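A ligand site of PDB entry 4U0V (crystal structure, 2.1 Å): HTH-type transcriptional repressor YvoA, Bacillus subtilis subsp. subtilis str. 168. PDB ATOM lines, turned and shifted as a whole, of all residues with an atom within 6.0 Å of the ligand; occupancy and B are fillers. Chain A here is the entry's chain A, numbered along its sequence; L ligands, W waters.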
ATOM      1  N   THR A  90      -9.930  17.572  -6.740  1.00  0.00           N
ATOM      2  CA  THR A  90     -10.848  18.604  -6.272  1.00  0.00           C
ATOM      3  C   THR A  90     -11.446  19.389  -7.427  1.00  0.00           C
ATOM      4  O   THR A  90     -10.952  19.343  -8.549  1.00  0.00           O
ATOM      5  CB  THR A  90     -10.146  19.612  -5.348  1.00  0.00           C
ATOM      6  OG1 THR A  90      -9.147  20.295  -6.116  1.00  0.00           O
ATOM      7  CG2 THR A  90      -9.497  18.911  -4.135  1.00  0.00           C
ATOM      8  N   SER A  91     -12.489  20.155  -7.126  1.00  0.00           N
ATOM      9  CA  SER A  91     -13.051  21.115  -8.068  1.00  0.00           C
ATOM     10  C   SER A  91     -12.406  22.476  -7.899  1.00  0.00           C
ATOM     11  O   SER A  91     -11.835  22.787  -6.832  1.00  0.00           O
ATOM     12  CB  SER A  91     -14.560  21.231  -7.865  1.00  0.00           C
ATOM     13  OG  SER A  91     -14.807  21.957  -6.664  1.00  0.00           O
ATOM     14  N   PHE A  92     -12.507  23.299  -8.947  1.00  0.00           N
ATOM     15  CA  PHE A  92     -12.126  24.710  -8.882  1.00  0.00           C
ATOM     16  C   PHE A  92     -12.823  25.420  -7.737  1.00  0.00           C
ATOM     17  O   PHE A  92     -12.216  26.224  -7.022  1.00  0.00           O
ATOM     18  CB  PHE A  92     -12.463  25.407 -10.204  1.00  0.00           C
ATOM     19  CG  PHE A  92     -12.008  26.853 -10.260  1.00  0.00           C
ATOM     20  CD1 PHE A  92     -10.688  27.175 -10.561  1.00  0.00           C
ATOM     21  CD2 PHE A  92     -12.901  27.879 -10.020  1.00  0.00           C
ATOM     22  CE1 PHE A  92     -10.268  28.505 -10.632  1.00  0.00           C
ATOM     23  CE2 PHE A  92     -12.497  29.209 -10.080  1.00  0.00           C
ATOM     24  CZ  PHE A  92     -11.179  29.517 -10.384  1.00  0.00           C
ATOM     25  N   THR A  93     -14.111  25.113  -7.585  1.00  0.00           N
ATOM     26  CA  THR A  93     -14.937  25.712  -6.539  1.00  0.00           C
ATOM     27  C   THR A  93     -14.382  25.361  -5.161  1.00  0.00           C
ATOM     28  O   THR A  93     -14.234  26.239  -4.304  1.00  0.00           O
ATOM     29  CB  THR A  93     -16.425  25.266  -6.645  1.00  0.00           C
ATOM     30  OG1 THR A  93     -16.970  25.742  -7.884  1.00  0.00           O
ATOM     31  CG2 THR A  93     -17.253  25.849  -5.514  1.00  0.00           C
ATOM     32  N   GLU A  94     -14.055  24.091  -4.954  1.00  0.00           N
ATOM     33  CA  GLU A  94     -13.380  23.673  -3.720  1.00  0.00           C
ATOM     34  C   GLU A  94     -12.014  24.330  -3.580  1.00  0.00           C
ATOM     35  O   GLU A  94     -11.646  24.770  -2.489  1.00  0.00           O
ATOM     36  CB  GLU A  94     -13.211  22.154  -3.673  1.00  0.00           C
ATOM     37  CG  GLU A  94     -14.506  21.376  -3.551  1.00  0.00           C
ATOM     38  CD  GLU A  94     -14.313  19.877  -3.752  1.00  0.00           C
ATOM     39  OE1 GLU A  94     -15.064  19.100  -3.152  1.00  0.00           O
ATOM     40  OE2 GLU A  94     -13.409  19.465  -4.522  1.00  0.00           O
ATOM     41  N   ASP A  95     -11.269  24.396  -4.686  1.00  0.00           N
ATOM     42  CA  ASP A  95      -9.920  24.974  -4.660  1.00  0.00           C
ATOM     43  C   ASP A  95      -9.941  26.418  -4.189  1.00  0.00           C
ATOM     44  O   ASP A  95      -9.084  26.831  -3.395  1.00  0.00           O
ATOM     45  CB  ASP A  95      -9.238  24.908  -6.038  1.00  0.00           C
ATOM     46  CG  ASP A  95      -8.885  23.491  -6.483  1.00  0.00           C
ATOM     47  OD1 ASP A  95      -8.819  22.578  -5.628  1.00  0.00           O
ATOM     48  OD2 ASP A  95      -8.661  23.285  -7.699  1.00  0.00           O
ATOM     49  N   SER A 105     -17.567  31.821 -12.650  1.00  0.00           N
ATOM     50  CA  SER A 105     -17.399  31.381 -14.019  1.00  0.00           C
ATOM     51  C   SER A 105     -18.178  32.276 -14.979  1.00  0.00           C
ATOM     52  O   SER A 105     -19.210  32.836 -14.626  1.00  0.00           O
ATOM     53  CB  SER A 105     -17.874  29.934 -14.223  1.00  0.00           C
ATOM     54  OG  SER A 105     -17.113  29.016 -13.450  1.00  0.00           O
ATOM     55  N   ARG A 136     -15.791  27.158 -20.100  1.00  0.00           N
ATOM     56  CA  ARG A 136     -15.938  28.258 -19.159  1.00  0.00           C
ATOM     57  C   ARG A 136     -14.604  28.894 -18.836  1.00  0.00           C
ATOM     58  O   ARG A 136     -13.575  28.221 -18.839  1.00  0.00           O
ATOM     59  CB  ARG A 136     -16.591  27.776 -17.848  1.00  0.00           C
ATOM     60  CG  ARG A 136     -17.970  27.113 -17.990  1.00  0.00           C
ATOM     61  CD  ARG A 136     -18.539  26.688 -16.608  1.00  0.00           C
ATOM     62  NE  ARG A 136     -17.807  25.557 -16.037  1.00  0.00           N
ATOM     63  CZ  ARG A 136     -17.850  25.187 -14.755  1.00  0.00           C
ATOM     64  NH1 ARG A 136     -18.595  25.856 -13.877  1.00  0.00           N
ATOM     65  NH2 ARG A 136     -17.147  24.147 -14.351  1.00  0.00           N
ATOM     66  N   ARG A 138     -12.777  30.395 -15.608  1.00  0.00           N
ATOM     67  CA  ARG A 138     -12.949  30.259 -14.176  1.00  0.00           C
ATOM     68  C   ARG A 138     -12.268  31.427 -13.477  1.00  0.00           C
ATOM     69  O   ARG A 138     -11.092  31.719 -13.758  1.00  0.00           O
ATOM     70  CB  ARG A 138     -12.384  28.937 -13.673  1.00  0.00           C
ATOM     71  CG  ARG A 138     -12.666  27.725 -14.551  1.00  0.00           C
ATOM     72  CD  ARG A 138     -14.173  27.461 -14.773  1.00  0.00           C
ATOM     73  NE  ARG A 138     -14.964  27.435 -13.537  1.00  0.00           N
ATOM     74  CZ  ARG A 138     -15.102  26.363 -12.751  1.00  0.00           C
ATOM     75  NH1 ARG A 138     -14.461  25.228 -13.022  1.00  0.00           N
ATOM     76  NH2 ARG A 138     -15.854  26.447 -11.671  1.00  0.00           N
ATOM     77  N   GLU A 148     -11.553  26.223 -19.221  1.00  0.00           N
ATOM     78  CA  GLU A 148     -11.765  24.781 -19.146  1.00  0.00           C
ATOM     79  C   GLU A 148     -12.875  24.344 -20.080  1.00  0.00           C
ATOM     80  O   GLU A 148     -13.945  24.948 -20.066  1.00  0.00           O
ATOM     81  CB  GLU A 148     -12.130  24.376 -17.732  1.00  0.00           C
ATOM     82  CG  GLU A 148     -11.141  24.884 -16.672  1.00  0.00           C
ATOM     83  CD  GLU A 148     -11.297  24.154 -15.362  1.00  0.00           C
ATOM     84  OE1 GLU A 148     -12.419  24.182 -14.806  1.00  0.00           O
ATOM     85  OE2 GLU A 148     -10.317  23.538 -14.888  1.00  0.00           O
ATOM     86  N   SER A 150     -15.047  21.050 -20.666  1.00  0.00           N
ATOM     87  CA  SER A 150     -15.353  19.776 -20.054  1.00  0.00           C
ATOM     88  C   SER A 150     -16.387  19.043 -20.879  1.00  0.00           C
ATOM     89  O   SER A 150     -17.474  19.564 -21.121  1.00  0.00           O
ATOM     90  CB  SER A 150     -15.837  19.981 -18.617  1.00  0.00           C
ATOM     91  OG  SER A 150     -16.267  18.759 -18.047  1.00  0.00           O
ATOM     92  N   HIS A 164     -26.258  25.932 -13.479  1.00  0.00           N
ATOM     93  CA  HIS A 164     -25.232  24.902 -13.347  1.00  0.00           C
ATOM     94  C   HIS A 164     -23.888  25.490 -13.770  1.00  0.00           C
ATOM     95  O   HIS A 164     -22.864  25.309 -13.089  1.00  0.00           O
ATOM     96  CB  HIS A 164     -25.551  23.660 -14.190  1.00  0.00           C
ATOM     97  CG  HIS A 164     -26.825  22.970 -13.806  1.00  0.00           C
ATOM     98  ND1 HIS A 164     -27.986  23.058 -14.566  1.00  0.00           N
ATOM     99  CD2 HIS A 164     -27.129  22.161 -12.766  1.00  0.00           C
ATOM    100  CE1 HIS A 164     -28.934  22.352 -13.988  1.00  0.00           C
ATOM    101  NE2 HIS A 164     -28.447  21.806 -12.887  1.00  0.00           N
ATOM    102  N   SER A 167     -22.123  27.777 -11.215  1.00  0.00           N
ATOM    103  CA  SER A 167     -21.669  27.199  -9.950  1.00  0.00           C
ATOM    104  C   SER A 167     -20.750  25.981 -10.187  1.00  0.00           C
ATOM    105  O   SER A 167     -19.922  25.988 -11.103  1.00  0.00           O
ATOM    106  CB  SER A 167     -22.868  26.804  -9.084  1.00  0.00           C
ATOM    107  OG  SER A 167     -23.794  26.024  -9.803  1.00  0.00           O
ATOM    108  N   SER A 168     -20.871  24.949  -9.358  1.00  0.00           N
ATOM    109  CA  SER A 168     -19.896  23.861  -9.389  1.00  0.00           C
ATOM    110  C   SER A 168     -20.424  22.661 -10.167  1.00  0.00           C
ATOM    111  O   SER A 168     -21.453  22.091  -9.813  1.00  0.00           O
ATOM    112  CB  SER A 168     -19.505  23.450  -7.968  1.00  0.00           C
ATOM    113  OG  SER A 168     -18.925  22.159  -7.975  1.00  0.00           O
ATOM    114  N   ILE A 169     -19.726  22.299 -11.238  1.00  0.00           N
ATOM    115  CA  ILE A 169     -20.176  21.163 -12.061  1.00  0.00           C
ATOM    116  C   ILE A 169     -19.976  19.858 -11.294  1.00  0.00           C
ATOM    117  O   ILE A 169     -20.819  18.944 -11.361  1.00  0.00           O
ATOM    118  CB  ILE A 169     -19.430  21.124 -13.432  1.00  0.00           C
ATOM    119  CG1 ILE A 169     -19.888  22.296 -14.293  1.00  0.00           C
ATOM    120  CG2 ILE A 169     -19.708  19.813 -14.163  1.00  0.00           C
ATOM    121  CD1 ILE A 169     -21.387  22.193 -14.732  1.00  0.00           C
ATOM    122  N   TYR A 170     -18.881  19.768 -10.560  1.00  0.00           N
ATOM    123  CA  TYR A 170     -18.603  18.565  -9.768  1.00  0.00           C
ATOM    124  C   TYR A 170     -19.662  18.355  -8.695  1.00  0.00           C
ATOM    125  O   TYR A 170     -20.091  17.228  -8.460  1.00  0.00           O
ATOM    126  CB  TYR A 170     -17.228  18.638  -9.121  1.00  0.00           C
ATOM    127  CG  TYR A 170     -16.078  18.243 -10.028  1.00  0.00           C
ATOM    128  CD1 TYR A 170     -14.833  17.955  -9.500  1.00  0.00           C
ATOM    129  CD2 TYR A 170     -16.226  18.191 -11.413  1.00  0.00           C
ATOM    130  CE1 TYR A 170     -13.769  17.609 -10.301  1.00  0.00           C
ATOM    131  CE2 TYR A 170     -15.156  17.821 -12.242  1.00  0.00           C
ATOM    132  CZ  TYR A 170     -13.926  17.541 -11.667  1.00  0.00           C
ATOM    133  OH  TYR A 170     -12.834  17.192 -12.426  1.00  0.00           O
ATOM    134  N   ASP A 171     -20.071  19.450  -8.032  1.00  0.00           N
ATOM    135  CA  ASP A 171     -21.207  19.380  -7.089  1.00  0.00           C
ATOM    136  C   ASP A 171     -22.438  18.766  -7.758  1.00  0.00           C
ATOM    137  O   ASP A 171     -23.043  17.828  -7.247  1.00  0.00           O
ATOM    138  CB  ASP A 171     -21.547  20.768  -6.572  1.00  0.00           C
ATOM    139  CG  ASP A 171     -22.167  20.739  -5.191  1.00  0.00           C
ATOM    140  OD1 ASP A 171     -23.296  21.269  -5.051  1.00  0.00           O
ATOM    141  OD2 ASP A 171     -21.540  20.211  -4.242  1.00  0.00           O
ATOM    142  N   GLN A 186      -4.453  12.904 -15.067  1.00  0.00           N
ATOM    143  CA  GLN A 186      -4.141  14.163 -15.757  1.00  0.00           C
ATOM    144  C   GLN A 186      -2.863  14.085 -16.582  1.00  0.00           C
ATOM    145  O   GLN A 186      -1.897  13.415 -16.199  1.00  0.00           O
ATOM    146  CB  GLN A 186      -4.035  15.349 -14.783  1.00  0.00           C
ATOM    147  CG  GLN A 186      -5.350  15.819 -14.224  1.00  0.00           C
ATOM    148  CD  GLN A 186      -5.304  17.211 -13.585  1.00  0.00           C
ATOM    149  OE1 GLN A 186      -6.308  17.920 -13.597  1.00  0.00           O
ATOM    150  NE2 GLN A 186      -4.159  17.592 -13.006  1.00  0.00           N
ATOM    151  N   ARG A 214      -7.694  16.195 -18.290  1.00  0.00           N
ATOM    152  CA  ARG A 214      -8.140  15.441 -17.139  1.00  0.00           C
ATOM    153  C   ARG A 214      -9.225  14.450 -17.542  1.00  0.00           C
ATOM    154  O   ARG A 214     -10.164  14.816 -18.223  1.00  0.00           O
ATOM    155  CB  ARG A 214      -8.677  16.390 -16.059  1.00  0.00           C
ATOM    156  CG  ARG A 214      -9.245  15.656 -14.855  1.00  0.00           C
ATOM    157  CD  ARG A 214      -9.842  16.603 -13.847  1.00  0.00           C
ATOM    158  NE  ARG A 214      -8.789  17.315 -13.119  1.00  0.00           N
ATOM    159  CZ  ARG A 214      -8.987  17.974 -11.987  1.00  0.00           C
ATOM    160  NH1 ARG A 214     -10.200  18.033 -11.422  1.00  0.00           N
ATOM    161  NH2 ARG A 214      -7.968  18.603 -11.415  1.00  0.00           N
ATOM    162  N   THR A 216     -11.832  12.050 -15.606  1.00  0.00           N
ATOM    163  CA  THR A 216     -12.283  11.951 -14.228  1.00  0.00           C
ATOM    164  C   THR A 216     -13.346  10.857 -14.033  1.00  0.00           C
ATOM    165  O   THR A 216     -14.227  10.681 -14.879  1.00  0.00           O
ATOM    166  CB  THR A 216     -12.822  13.294 -13.771  1.00  0.00           C
ATOM    167  OG1 THR A 216     -12.071  14.341 -14.423  1.00  0.00           O
ATOM    168  CG2 THR A 216     -12.734  13.438 -12.259  1.00  0.00           C
ATOM    169  N   GLU A 225     -16.090  12.653 -17.120  1.00  0.00           N
ATOM    170  CA  GLU A 225     -15.555  13.894 -17.661  1.00  0.00           C
ATOM    171  C   GLU A 225     -14.263  13.660 -18.430  1.00  0.00           C
ATOM    172  O   GLU A 225     -13.379  12.929 -17.973  1.00  0.00           O
ATOM    173  CB  GLU A 225     -15.290  14.903 -16.526  1.00  0.00           C
ATOM    174  CG  GLU A 225     -14.486  16.124 -16.975  1.00  0.00           C
ATOM    175  CD  GLU A 225     -14.106  17.037 -15.830  1.00  0.00           C
ATOM    176  OE1 GLU A 225     -14.400  18.239 -15.919  1.00  0.00           O
ATOM    177  OE2 GLU A 225     -13.500  16.548 -14.839  1.00  0.00           O
ATOM    178  N   ALA A 227     -11.790  16.600 -19.817  1.00  0.00           N
ATOM    179  CA  ALA A 227     -11.647  18.058 -19.814  1.00  0.00           C
ATOM    180  C   ALA A 227     -10.290  18.508 -20.326  1.00  0.00           C
ATOM    181  O   ALA A 227      -9.270  17.881 -20.058  1.00  0.00           O
ATOM    182  CB  ALA A 227     -11.864  18.603 -18.392  1.00  0.00           C
ATOM    183  N   SER A 229      -7.993  21.995 -20.336  1.00  0.00           N
ATOM    184  CA  SER A 229      -7.912  23.300 -19.681  1.00  0.00           C
ATOM    185  C   SER A 229      -6.572  23.963 -19.916  1.00  0.00           C
ATOM    186  O   SER A 229      -5.565  23.273 -20.093  1.00  0.00           O
ATOM    187  CB  SER A 229      -8.138  23.164 -18.169  1.00  0.00           C
ATOM    188  OG  SER A 229      -9.174  22.260 -17.881  1.00  0.00           O
ATOM    189  N   TYR A 231      -4.255  26.785 -17.808  1.00  0.00           N
ATOM    190  CA  TYR A 231      -4.074  27.546 -16.567  1.00  0.00           C
ATOM    191  C   TYR A 231      -3.000  28.603 -16.727  1.00  0.00           C
ATOM    192  O   TYR A 231      -1.937  28.326 -17.264  1.00  0.00           O
ATOM    193  CB  TYR A 231      -3.717  26.604 -15.427  1.00  0.00           C
ATOM    194  CG  TYR A 231      -4.896  25.820 -14.905  1.00  0.00           C
ATOM    195  CD1 TYR A 231      -5.538  26.210 -13.750  1.00  0.00           C
ATOM    196  CD2 TYR A 231      -5.377  24.707 -15.595  1.00  0.00           C
ATOM    197  CE1 TYR A 231      -6.623  25.523 -13.267  1.00  0.00           C
ATOM    198  CE2 TYR A 231      -6.472  24.006 -15.108  1.00  0.00           C
ATOM    199  CZ  TYR A 231      -7.084  24.435 -13.946  1.00  0.00           C
ATOM    200  OH  TYR A 231      -8.156  23.750 -13.444  1.00  0.00           O
HETATM  201  C1  LIG L   1     -11.141  21.685 -11.829  1.00  0.00           C
HETATM  202  C2  LIG L   1     -10.768  20.780 -13.005  1.00  0.00           C
HETATM  203  C3  LIG L   1     -11.765  20.719 -14.092  1.00  0.00           C
HETATM  204  C4  LIG L   1     -13.149  20.519 -13.584  1.00  0.00           C
HETATM  205  C5  LIG L   1     -13.460  21.659 -12.634  1.00  0.00           C
HETATM  206  C6  LIG L   1     -14.863  21.606 -12.082  1.00  0.00           C
HETATM  207  O1  LIG L   1     -10.886  23.002 -12.124  1.00  0.00           O
HETATM  208  N1  LIG L   1      -9.510  21.229 -13.608  1.00  0.00           N
HETATM  209  O2  LIG L   1     -11.391  19.591 -14.950  1.00  0.00           O
HETATM  210  O3  LIG L   1     -14.056  20.485 -14.681  1.00  0.00           O
HETATM  211  O4  LIG L   1     -12.577  21.593 -11.485  1.00  0.00           O
HETATM  212  O5  LIG L   1     -14.954  22.692 -11.183  1.00  0.00           O
HETATM  213  P1  LIG L   1     -16.423  23.111 -10.638  1.00  0.00           P
HETATM  214  O6  LIG L   1     -16.236  24.326  -9.756  1.00  0.00           O
HETATM  215  O7  LIG L   1     -17.036  21.954  -9.908  1.00  0.00           O
HETATM  216  O8  LIG L   1     -17.374  23.433 -11.797  1.00  0.00           O
HETATM  217  O   HOH W   1     -14.775  22.887 -15.848  1.00  0.00           O
HETATM  218  O   HOH W   2      -7.690  19.995 -15.080  1.00  0.00           O
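Merely in contact with the ligand: Ser 91 (3.3 Å), Ser 167 (3.7 Å), Arg 214 (3.2 Å) and Ala 227 (3.6 Å). Hydrophobic or aromatic side chains that line the ligand: Phe 92, Ile 169, Tyr 170 and Ala 227. Of the 24 residues printed, 14 come within 4 Å of the ligand.
Water W2 lies within hydrogen-bond range of a nitrogen (N1) of the ligand (2.6 Å), the side-chain amide oxygen (OE1) of Gln 186 (2.9 Å) and the guanidinium group (NE) of Arg 214 (3.5 Å). Water W1 lies within hydrogen-bond range of O3 of the ligand, OE1 of Glu 148 and NH2 of Arg 136.
The backbone NH of Thr 93 lies within hydrogen-bond range of an oxygen (O6) of the ligand, 3.1 Å away. An oxygen (O6) of the ligand is in hydrogen-bond range of the side-chain hydroxyl (OG1) of Thr 93 (2.5 Å). O3 of the ligand is in hydrogen-bond range of OE1 of Glu 225 (2.6 Å). The guanidinium group of Arg 136 is in salt-bridge range of an oxygen (O8) of the ligand (2.7 Å). O8 of the ligand sits at hydrogen-bond distance from N of Ile 169, 2.7 Å away. OG of Ser 168 is in hydrogen-bond range of O7 of the ligand (2.7 Å). The side-chain carboxylate of Glu 148 lies within salt-bridge range of a nitrogen (N1) of the ligand, at 2.8 Å. The side-chain hydroxyl of Tyr 231 lies within hydrogen-bond range of a nitrogen (N1) of the ligand (2.9 Å). NH2 of Arg 138 lies within salt-bridge range of O6 of the ligand, 2.9 Å away. The backbone NH of Tyr 170 is in hydrogen-bond range of an oxygen (O7) of the ligand (2.9 Å). N of Phe 92 is in hydrogen-bond range of O4 of the ligand (3.1 Å).
The side-chain hydroxyl of Ser 91 lies close to the backbone NH of Thr 93 (3.4 Å). OE2 of Glu 225 is in hydrogen-bond range of OH of Tyr 170 (2.6 Å). The side-chain carboxylate (OE2) of Glu 225 sits at hydrogen-bond distance from the side-chain hydroxyl (OG1) of Thr 216 (2.7 Å). The backbone NH of Glu 148 lies within hydrogen-bond range of the backbone carbonyl oxygen of Arg 136 (2.9 Å). OG of Ser 168 sits at hydrogen-bond distance from N of Asp 171 (2.9 Å). OE2 of Glu 148 sits at hydrogen-bond distance from OH of Tyr 231, 2.6 Å away. The backbone NH (N) of Ala 227 is in hydrogen-bond range of the backbone carbonyl oxygen (O) of Arg 214. O of Thr 90 is in hydrogen-bond range of NH1 of Arg 214.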
